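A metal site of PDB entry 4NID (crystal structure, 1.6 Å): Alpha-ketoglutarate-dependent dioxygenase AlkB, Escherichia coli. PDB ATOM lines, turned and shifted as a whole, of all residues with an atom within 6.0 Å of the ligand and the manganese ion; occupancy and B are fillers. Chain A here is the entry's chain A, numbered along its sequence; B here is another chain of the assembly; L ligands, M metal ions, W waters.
The guanidinium group (NH1) of Arg 193 lies within salt-bridge range of an oxygen (O5) of the ligand. ND2 of Asn 195 sits at hydrogen-bond distance from O4 of the ligand, at 3.1 Å. O2 of the ligand lies close to OD1 of Asn 109, at 2.8 Å. An oxygen (O5) of the ligand is in hydrogen-bond range of the side-chain hydroxyl (OH) of Tyr 111 (2.7 Å).
The backbone NH of Tyr 111 sits at hydrogen-bond distance from the backbone carbonyl oxygen of Arg 193 (2.7 Å). ND2 of Asn 195 lies close to NH2 of Arg 193. N of Asn 195 sits at hydrogen-bond distance from O of Asn 109, at 2.9 Å. The backbone carbonyl oxygen (O) of Leu 107 sits at hydrogen-bond distance from the backbone NH (N) of Thr 197, at 2.8 Å. The side-chain amide nitrogen (ND2) of Asn 195 sits at hydrogen-bond distance from the side-chain hydroxyl (OG) of Ser 134. ND1 of His 120 lies within hydrogen-bond range of O4' of 6MA 8 of chain B, at 3.5 Å. SD of Met 50 sits close to ND2 of Asn 109, at 3.7 Å. The backbone NH of Ile 178 lies within hydrogen-bond range of the backbone carbonyl oxygen of Leu 117.
N1 of 6MA 8 of chain B lies close to O1 of the ligand, at 3.3 Å. Leu 107 touches the ligand. Leu 117 touches the ligand. Ser 134 touches the ligand. Ile 178 touches the ligand. Thr 197 touches the ligand (OG1 to O2, 3.7 Å). Hydrophobic or aromatic side chains that line the ligand: Leu 107, Tyr 111, Leu 117, His 120, His 176 and Ile 178. Within 4 Å of the ligand: Leu 107, Asn 109, Tyr 111, Leu 117, His 120, Asp 122, Ser 134, His 176, Ile 178, Arg 193, Asn 195, Thr 197 and 6MA 8 of chain B. The nearest printed residue that does not touch the ligand is Phe 143 (4.2 Å).
Of the 20 residues printed, 3 come within 4 Å of the manganese ion. The nearest printed residue that does not touch the manganese ion is 6MA 8 of chain B (4.3 Å).
The manganese ion is bound by the side-chain carboxylate of Asp 122 (2.1 Å), a ring nitrogen (NE2) of His 120 (2.2 Å), an oxygen (O1) of the ligand (2.2 Å), a ring nitrogen (NE2) of His 176 (2.2 Å), an oxygen (O3) of the ligand (2.4 Å) and water W1 (2.4 Å).
Water W2 bridges N1 of 6MA 8 of chain B and the side-chain carboxylate (OD2) of Asp 122. Water W4 bridges O4 of the ligand (2.7 Å) and OG of Ser 134 (2.7 Å). Water W3 lies within hydrogen-bond range of the side-chain hydroxyl of Thr 197 (2.7 Å) and the side-chain hydroxyl of Ser 134 (2.8 Å).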
ATOM      1  N   MET A  50      15.152  12.232  -9.413  1.00  0.00           N
ATOM      2  CA  MET A  50      16.494  12.477  -9.963  1.00  0.00           C
ATOM      3  C   MET A  50      16.415  12.973 -11.409  1.00  0.00           C
ATOM      4  O   MET A  50      15.468  12.662 -12.132  1.00  0.00           O
ATOM      5  CB  MET A  50      17.328  11.207  -9.903  1.00  0.00           C
ATOM      6  CG  MET A  50      17.715  10.842  -8.477  1.00  0.00           C
ATOM      7  SD  MET A  50      18.509   9.235  -8.431  1.00  0.00           S
ATOM      8  CE  MET A  50      19.407   9.242  -6.881  1.00  0.00           C
ATOM      9  N   LEU A 107      24.567  14.371 -11.151  1.00  0.00           N
ATOM     10  CA  LEU A 107      23.286  13.818 -10.737  1.00  0.00           C
ATOM     11  C   LEU A 107      22.590  14.884  -9.895  1.00  0.00           C
ATOM     12  O   LEU A 107      23.180  15.410  -8.942  1.00  0.00           O
ATOM     13  CB  LEU A 107      23.515  12.542  -9.940  1.00  0.00           C
ATOM     14  CG  LEU A 107      22.329  11.863  -9.258  1.00  0.00           C
ATOM     15  CD1 LEU A 107      21.291  11.480 -10.301  1.00  0.00           C
ATOM     16  CD2 LEU A 107      22.807  10.627  -8.503  1.00  0.00           C
ATOM     17  N   ASN A 109      19.466  15.663  -7.414  1.00  0.00           N
ATOM     18  CA  ASN A 109      18.560  14.950  -6.514  1.00  0.00           C
ATOM     19  C   ASN A 109      17.572  15.942  -5.917  1.00  0.00           C
ATOM     20  O   ASN A 109      17.976  17.004  -5.477  1.00  0.00           O
ATOM     21  CB  ASN A 109      19.350  14.253  -5.376  1.00  0.00           C
ATOM     22  CG  ASN A 109      20.325  13.196  -5.883  1.00  0.00           C
ATOM     23  OD1 ASN A 109      21.519  13.239  -5.584  1.00  0.00           O
ATOM     24  ND2 ASN A 109      19.817  12.238  -6.625  1.00  0.00           N
ATOM     25  N   TYR A 111      14.663  16.177  -2.970  1.00  0.00           N
ATOM     26  CA  TYR A 111      14.080  15.551  -1.781  1.00  0.00           C
ATOM     27  C   TYR A 111      12.841  16.294  -1.338  1.00  0.00           C
ATOM     28  O   TYR A 111      12.937  17.456  -0.927  1.00  0.00           O
ATOM     29  CB  TYR A 111      15.083  15.573  -0.612  1.00  0.00           C
ATOM     30  CG  TYR A 111      16.334  14.766  -0.824  1.00  0.00           C
ATOM     31  CD1 TYR A 111      17.386  15.258  -1.604  1.00  0.00           C
ATOM     32  CD2 TYR A 111      16.488  13.525  -0.207  1.00  0.00           C
ATOM     33  CE1 TYR A 111      18.556  14.520  -1.772  1.00  0.00           C
ATOM     34  CE2 TYR A 111      17.643  12.787  -0.382  1.00  0.00           C
ATOM     35  CZ  TYR A 111      18.649  13.283  -1.174  1.00  0.00           C
ATOM     36  OH  TYR A 111      19.770  12.498  -1.321  1.00  0.00           O
ATOM     37  N   LEU A 117      17.885   8.658   1.218  1.00  0.00           N
ATOM     38  CA  LEU A 117      18.775   7.876   0.368  1.00  0.00           C
ATOM     39  C   LEU A 117      19.561   6.968   1.301  1.00  0.00           C
ATOM     40  O   LEU A 117      20.420   7.427   2.063  1.00  0.00           O
ATOM     41  CB  LEU A 117      19.669   8.805  -0.471  1.00  0.00           C
ATOM     42  CG  LEU A 117      20.400   8.233  -1.677  1.00  0.00           C
ATOM     43  CD1 LEU A 117      19.473   7.492  -2.637  1.00  0.00           C
ATOM     44  CD2 LEU A 117      21.167   9.323  -2.419  1.00  0.00           C
ATOM     45  N   HIS A 120      24.896   3.865   1.033  1.00  0.00           N
ATOM     46  CA  HIS A 120      25.374   3.283  -0.189  1.00  0.00           C
ATOM     47  C   HIS A 120      26.790   3.784  -0.433  1.00  0.00           C
ATOM     48  O   HIS A 120      27.283   4.679   0.252  1.00  0.00           O
ATOM     49  CB  HIS A 120      24.465   3.622  -1.392  1.00  0.00           C
ATOM     50  CG  HIS A 120      24.482   5.073  -1.768  1.00  0.00           C
ATOM     51  ND1 HIS A 120      23.677   5.988  -1.131  1.00  0.00           N
ATOM     52  CD2 HIS A 120      25.216   5.761  -2.667  1.00  0.00           C
ATOM     53  CE1 HIS A 120      23.908   7.191  -1.635  1.00  0.00           C
ATOM     54  NE2 HIS A 120      24.829   7.089  -2.574  1.00  0.00           N
ATOM     55  N   GLN A 121      27.466   3.162  -1.397  1.00  0.00           N
ATOM     56  CA  GLN A 121      28.753   3.655  -1.873  1.00  0.00           C
ATOM     57  C   GLN A 121      28.594   4.132  -3.298  1.00  0.00           C
ATOM     58  O   GLN A 121      27.802   3.561  -4.051  1.00  0.00           O
ATOM     59  CB  GLN A 121      29.786   2.522  -1.875  1.00  0.00           C
ATOM     60  CG  GLN A 121      30.042   1.801  -0.543  1.00  0.00           C
ATOM     61  CD  GLN A 121      30.886   0.547  -0.740  1.00  0.00           C
ATOM     62  OE1 GLN A 121      30.391  -0.495  -1.185  1.00  0.00           O
ATOM     63  NE2 GLN A 121      32.180   0.650  -0.434  1.00  0.00           N
ATOM     64  N   ASP A 122      29.320   5.178  -3.677  1.00  0.00           N
ATOM     65  CA  ASP A 122      29.457   5.547  -5.080  1.00  0.00           C
ATOM     66  C   ASP A 122      30.635   4.731  -5.620  1.00  0.00           C
ATOM     67  O   ASP A 122      31.794   5.074  -5.440  1.00  0.00           O
ATOM     68  CB  ASP A 122      29.697   7.072  -5.227  1.00  0.00           C
ATOM     69  CG  ASP A 122      28.430   7.914  -5.060  1.00  0.00           C
ATOM     70  OD1 ASP A 122      27.549   7.583  -4.236  1.00  0.00           O
ATOM     71  OD2 ASP A 122      28.338   8.948  -5.762  1.00  0.00           O
ATOM     72  N   SER A 134      29.669  17.238  -3.737  1.00  0.00           N
ATOM     73  CA  SER A 134      28.260  17.104  -3.406  1.00  0.00           C
ATOM     74  C   SER A 134      27.750  18.447  -2.819  1.00  0.00           C
ATOM     75  O   SER A 134      28.190  18.849  -1.746  1.00  0.00           O
ATOM     76  CB  SER A 134      28.090  15.925  -2.408  1.00  0.00           C
ATOM     77  OG  SER A 134      26.733  15.561  -2.227  1.00  0.00           O
ATOM     78  N   SER A 136      24.644  20.952  -1.451  1.00  0.00           N
ATOM     79  CA  SER A 136      23.295  20.952  -0.837  1.00  0.00           C
ATOM     80  C   SER A 136      22.637  22.286  -1.095  1.00  0.00           C
ATOM     81  O   SER A 136      23.293  23.326  -0.945  1.00  0.00           O
ATOM     82  CB  SER A 136      23.399  20.810   0.685  1.00  0.00           C
ATOM     83  OG  SER A 136      23.938  19.543   1.027  1.00  0.00           O
ATOM     84  N   PHE A 143      23.115  14.053   6.896  1.00  0.00           N
ATOM     85  CA  PHE A 143      23.987  13.270   6.029  1.00  0.00           C
ATOM     86  C   PHE A 143      24.716  12.281   6.897  1.00  0.00           C
ATOM     87  O   PHE A 143      25.254  12.640   7.948  1.00  0.00           O
ATOM     88  CB  PHE A 143      25.004  14.226   5.408  1.00  0.00           C
ATOM     89  CG  PHE A 143      25.991  13.581   4.456  1.00  0.00           C
ATOM     90  CD1 PHE A 143      25.563  12.948   3.293  1.00  0.00           C
ATOM     91  CD2 PHE A 143      27.360  13.719   4.685  1.00  0.00           C
ATOM     92  CE1 PHE A 143      26.490  12.388   2.408  1.00  0.00           C
ATOM     93  CE2 PHE A 143      28.278  13.189   3.796  1.00  0.00           C
ATOM     94  CZ  PHE A 143      27.834  12.522   2.665  1.00  0.00           C
ATOM     95  N   LEU A 159      23.487  19.047   6.892  1.00  0.00           N
ATOM     96  CA  LEU A 159      23.945  19.767   5.711  1.00  0.00           C
ATOM     97  C   LEU A 159      22.909  20.832   5.435  1.00  0.00           C
ATOM     98  O   LEU A 159      21.715  20.515   5.279  1.00  0.00           O
ATOM     99  CB  LEU A 159      24.079  18.844   4.499  1.00  0.00           C
ATOM    100  CG  LEU A 159      25.141  17.751   4.618  1.00  0.00           C
ATOM    101  CD1 LEU A 159      25.249  16.940   3.336  1.00  0.00           C
ATOM    102  CD2 LEU A 159      26.516  18.309   4.998  1.00  0.00           C
ATOM    103  N   TRP A 167      34.497  14.169  -1.103  1.00  0.00           N
ATOM    104  CA  TRP A 167      35.296  13.019  -0.665  1.00  0.00           C
ATOM    105  C   TRP A 167      36.032  12.355  -1.821  1.00  0.00           C
ATOM    106  O   TRP A 167      35.621  12.472  -2.979  1.00  0.00           O
ATOM    107  CB  TRP A 167      34.494  12.047   0.206  1.00  0.00           C
ATOM    108  CG  TRP A 167      33.282  11.359  -0.390  1.00  0.00           C
ATOM    109  CD1 TRP A 167      33.208  10.053  -0.807  1.00  0.00           C
ATOM    110  CD2 TRP A 167      31.966  11.901  -0.546  1.00  0.00           C
ATOM    111  NE1 TRP A 167      31.936   9.762  -1.234  1.00  0.00           N
ATOM    112  CE2 TRP A 167      31.151  10.883  -1.095  1.00  0.00           C
ATOM    113  CE3 TRP A 167      31.389  13.164  -0.294  1.00  0.00           C
ATOM    114  CZ2 TRP A 167      29.786  11.075  -1.385  1.00  0.00           C
ATOM    115  CZ3 TRP A 167      30.040  13.355  -0.578  1.00  0.00           C
ATOM    116  CH2 TRP A 167      29.250  12.319  -1.128  1.00  0.00           C
ATOM    117  N   HIS A 176      27.694   6.279   2.613  1.00  0.00           N
ATOM    118  CA  HIS A 176      27.077   7.510   3.006  1.00  0.00           C
ATOM    119  C   HIS A 176      25.593   7.476   2.622  1.00  0.00           C
ATOM    120  O   HIS A 176      25.158   6.607   1.866  1.00  0.00           O
ATOM    121  CB  HIS A 176      27.789   8.675   2.323  1.00  0.00           C
ATOM    122  CG  HIS A 176      27.768   8.572   0.845  1.00  0.00           C
ATOM    123  ND1 HIS A 176      28.636   7.770   0.140  1.00  0.00           N
ATOM    124  CD2 HIS A 176      26.915   9.089  -0.074  1.00  0.00           C
ATOM    125  CE1 HIS A 176      28.350   7.822  -1.147  1.00  0.00           C
ATOM    126  NE2 HIS A 176      27.312   8.622  -1.303  1.00  0.00           N
ATOM    127  N   GLY A 177      24.842   8.459   3.118  1.00  0.00           N
ATOM    128  CA  GLY A 177      23.397   8.464   2.916  1.00  0.00           C
ATOM    129  C   GLY A 177      22.748   9.719   3.478  1.00  0.00           C
ATOM    130  O   GLY A 177      23.418  10.565   4.104  1.00  0.00           O
ATOM    131  N   ILE A 178      21.447   9.824   3.234  1.00  0.00           N
ATOM    132  CA  ILE A 178      20.637  10.935   3.704  1.00  0.00           C
ATOM    133  C   ILE A 178      19.428  10.404   4.464  1.00  0.00           C
ATOM    134  O   ILE A 178      18.695   9.546   3.958  1.00  0.00           O
ATOM    135  CB  ILE A 178      20.190  11.823   2.514  1.00  0.00           C
ATOM    136  CG1 ILE A 178      21.384  12.597   1.895  1.00  0.00           C
ATOM    137  CG2 ILE A 178      19.080  12.780   2.947  1.00  0.00           C
ATOM    138  CD1 ILE A 178      21.897  13.784   2.702  1.00  0.00           C
ATOM    139  N   ARG A 193      14.668  19.898  -0.774  1.00  0.00           N
ATOM    140  CA  ARG A 193      16.114  19.991  -0.802  1.00  0.00           C
ATOM    141  C   ARG A 193      16.547  19.529  -2.166  1.00  0.00           C
ATOM    142  O   ARG A 193      15.998  18.565  -2.720  1.00  0.00           O
ATOM    143  CB  ARG A 193      16.721  19.086   0.273  1.00  0.00           C
ATOM    144  CG  ARG A 193      18.224  18.893   0.138  1.00  0.00           C
ATOM    145  CD  ARG A 193      18.775  18.178   1.352  1.00  0.00           C
ATOM    146  NE  ARG A 193      20.233  18.145   1.327  1.00  0.00           N
ATOM    147  CZ  ARG A 193      20.967  17.173   0.802  1.00  0.00           C
ATOM    148  NH1 ARG A 193      20.404  16.078   0.278  1.00  0.00           N
ATOM    149  NH2 ARG A 193      22.280  17.296   0.817  1.00  0.00           N
ATOM    150  N   ASN A 195      20.182  18.338  -4.261  1.00  0.00           N
ATOM    151  CA  ASN A 195      21.592  18.045  -4.147  1.00  0.00           C
ATOM    152  C   ASN A 195      22.201  17.866  -5.535  1.00  0.00           C
ATOM    153  O   ASN A 195      21.593  17.272  -6.385  1.00  0.00           O
ATOM    154  CB  ASN A 195      21.782  16.794  -3.305  1.00  0.00           C
ATOM    155  CG  ASN A 195      23.235  16.462  -3.108  1.00  0.00           C
ATOM    156  OD1 ASN A 195      23.790  15.681  -3.866  1.00  0.00           O
ATOM    157  ND2 ASN A 195      23.864  17.090  -2.134  1.00  0.00           N
ATOM    158  N   THR A 197      25.432  16.194  -7.389  1.00  0.00           N
ATOM    159  CA  THR A 197      26.559  15.262  -7.203  1.00  0.00           C
ATOM    160  C   THR A 197      27.355  15.223  -8.474  1.00  0.00           C
ATOM    161  O   THR A 197      26.874  14.734  -9.509  1.00  0.00           O
ATOM    162  CB  THR A 197      26.005  13.883  -6.843  1.00  0.00           C
ATOM    163  OG1 THR A 197      25.423  13.978  -5.537  1.00  0.00           O
ATOM    164  CG2 THR A 197      27.124  12.850  -6.801  1.00  0.00           C
ATOM    165  P   6MA B   8      22.372   0.092  -2.479  1.00  0.00           P
ATOM    166  OP1 6MA B   8      23.380   0.505  -1.604  1.00  0.00           O
ATOM    167  OP2 6MA B   8      22.646  -0.099  -3.804  1.00  0.00           O
ATOM    168  O5' 6MA B   8      21.186   1.250  -2.502  1.00  0.00           O
ATOM    169  C5' 6MA B   8      20.927   1.967  -1.398  1.00  0.00           C
ATOM    170  C4' 6MA B   8      20.236   3.253  -1.878  1.00  0.00           C
ATOM    171  O4' 6MA B   8      21.139   4.065  -2.527  1.00  0.00           O
ATOM    172  C3' 6MA B   8      19.086   3.005  -2.831  1.00  0.00           C
ATOM    173  O3' 6MA B   8      18.118   4.036  -2.843  1.00  0.00           O
ATOM    174  C2' 6MA B   8      19.786   3.213  -4.176  1.00  0.00           C
ATOM    175  C1' 6MA B   8      20.826   4.278  -3.863  1.00  0.00           C
ATOM    176  N9  6MA B   8      22.088   4.305  -4.631  1.00  0.00           N
ATOM    177  C8  6MA B   8      22.935   3.280  -4.731  1.00  0.00           C
ATOM    178  N7  6MA B   8      23.995   3.624  -5.419  1.00  0.00           N
ATOM    179  C5  6MA B   8      23.873   4.867  -5.772  1.00  0.00           C
ATOM    180  C6  6MA B   8      24.711   5.787  -6.503  1.00  0.00           C
ATOM    181  N1  6MA B   8      24.298   7.021  -6.625  1.00  0.00           N
ATOM    182  C2  6MA B   8      23.113   7.364  -6.129  1.00  0.00           C
ATOM    183  N3  6MA B   8      22.279   6.616  -5.446  1.00  0.00           N
ATOM    184  C4  6MA B   8      22.616   5.334  -5.204  1.00  0.00           C
ATOM    185  N6  6MA B   8      25.876   5.333  -6.981  1.00  0.00           N
ATOM    186  C1  6MA B   8      26.630   6.184  -7.867  1.00  0.00           C
HETATM  187  C1  LIG L   1      24.036  10.534  -4.338  1.00  0.00           C
HETATM  188  O1  LIG L   1      24.806   9.598  -4.691  1.00  0.00           O
HETATM  189  O2  LIG L   1      23.228  11.067  -5.135  1.00  0.00           O
HETATM  190  C2  LIG L   1      24.111  11.001  -2.960  1.00  0.00           C
HETATM  191  O3  LIG L   1      24.795  10.357  -2.155  1.00  0.00           O
HETATM  192  C3  LIG L   1      23.357  12.259  -2.543  1.00  0.00           C
HETATM  193  C4  LIG L   1      23.817  12.754  -1.170  1.00  0.00           C
HETATM  194  C5  LIG L   1      23.067  14.025  -0.788  1.00  0.00           C
HETATM  195  O4  LIG L   1      23.669  14.806  -0.018  1.00  0.00           O
HETATM  196  O5  LIG L   1      21.895  14.225  -1.195  1.00  0.00           O
HETATM  197 MN    MN M   1      26.142   8.721  -3.193  1.00  0.00          MN
HETATM  198  O   HOH W   1      27.504  10.587  -3.789  1.00  0.00           O
HETATM  199  O   HOH W   2      25.882   9.319  -7.151  1.00  0.00           O
HETATM  200  O   HOH W   3      26.529  12.943  -3.329  1.00  0.00           O
HETATM  201  O   HOH W   4      26.294  15.274   0.426  1.00  0.00           O
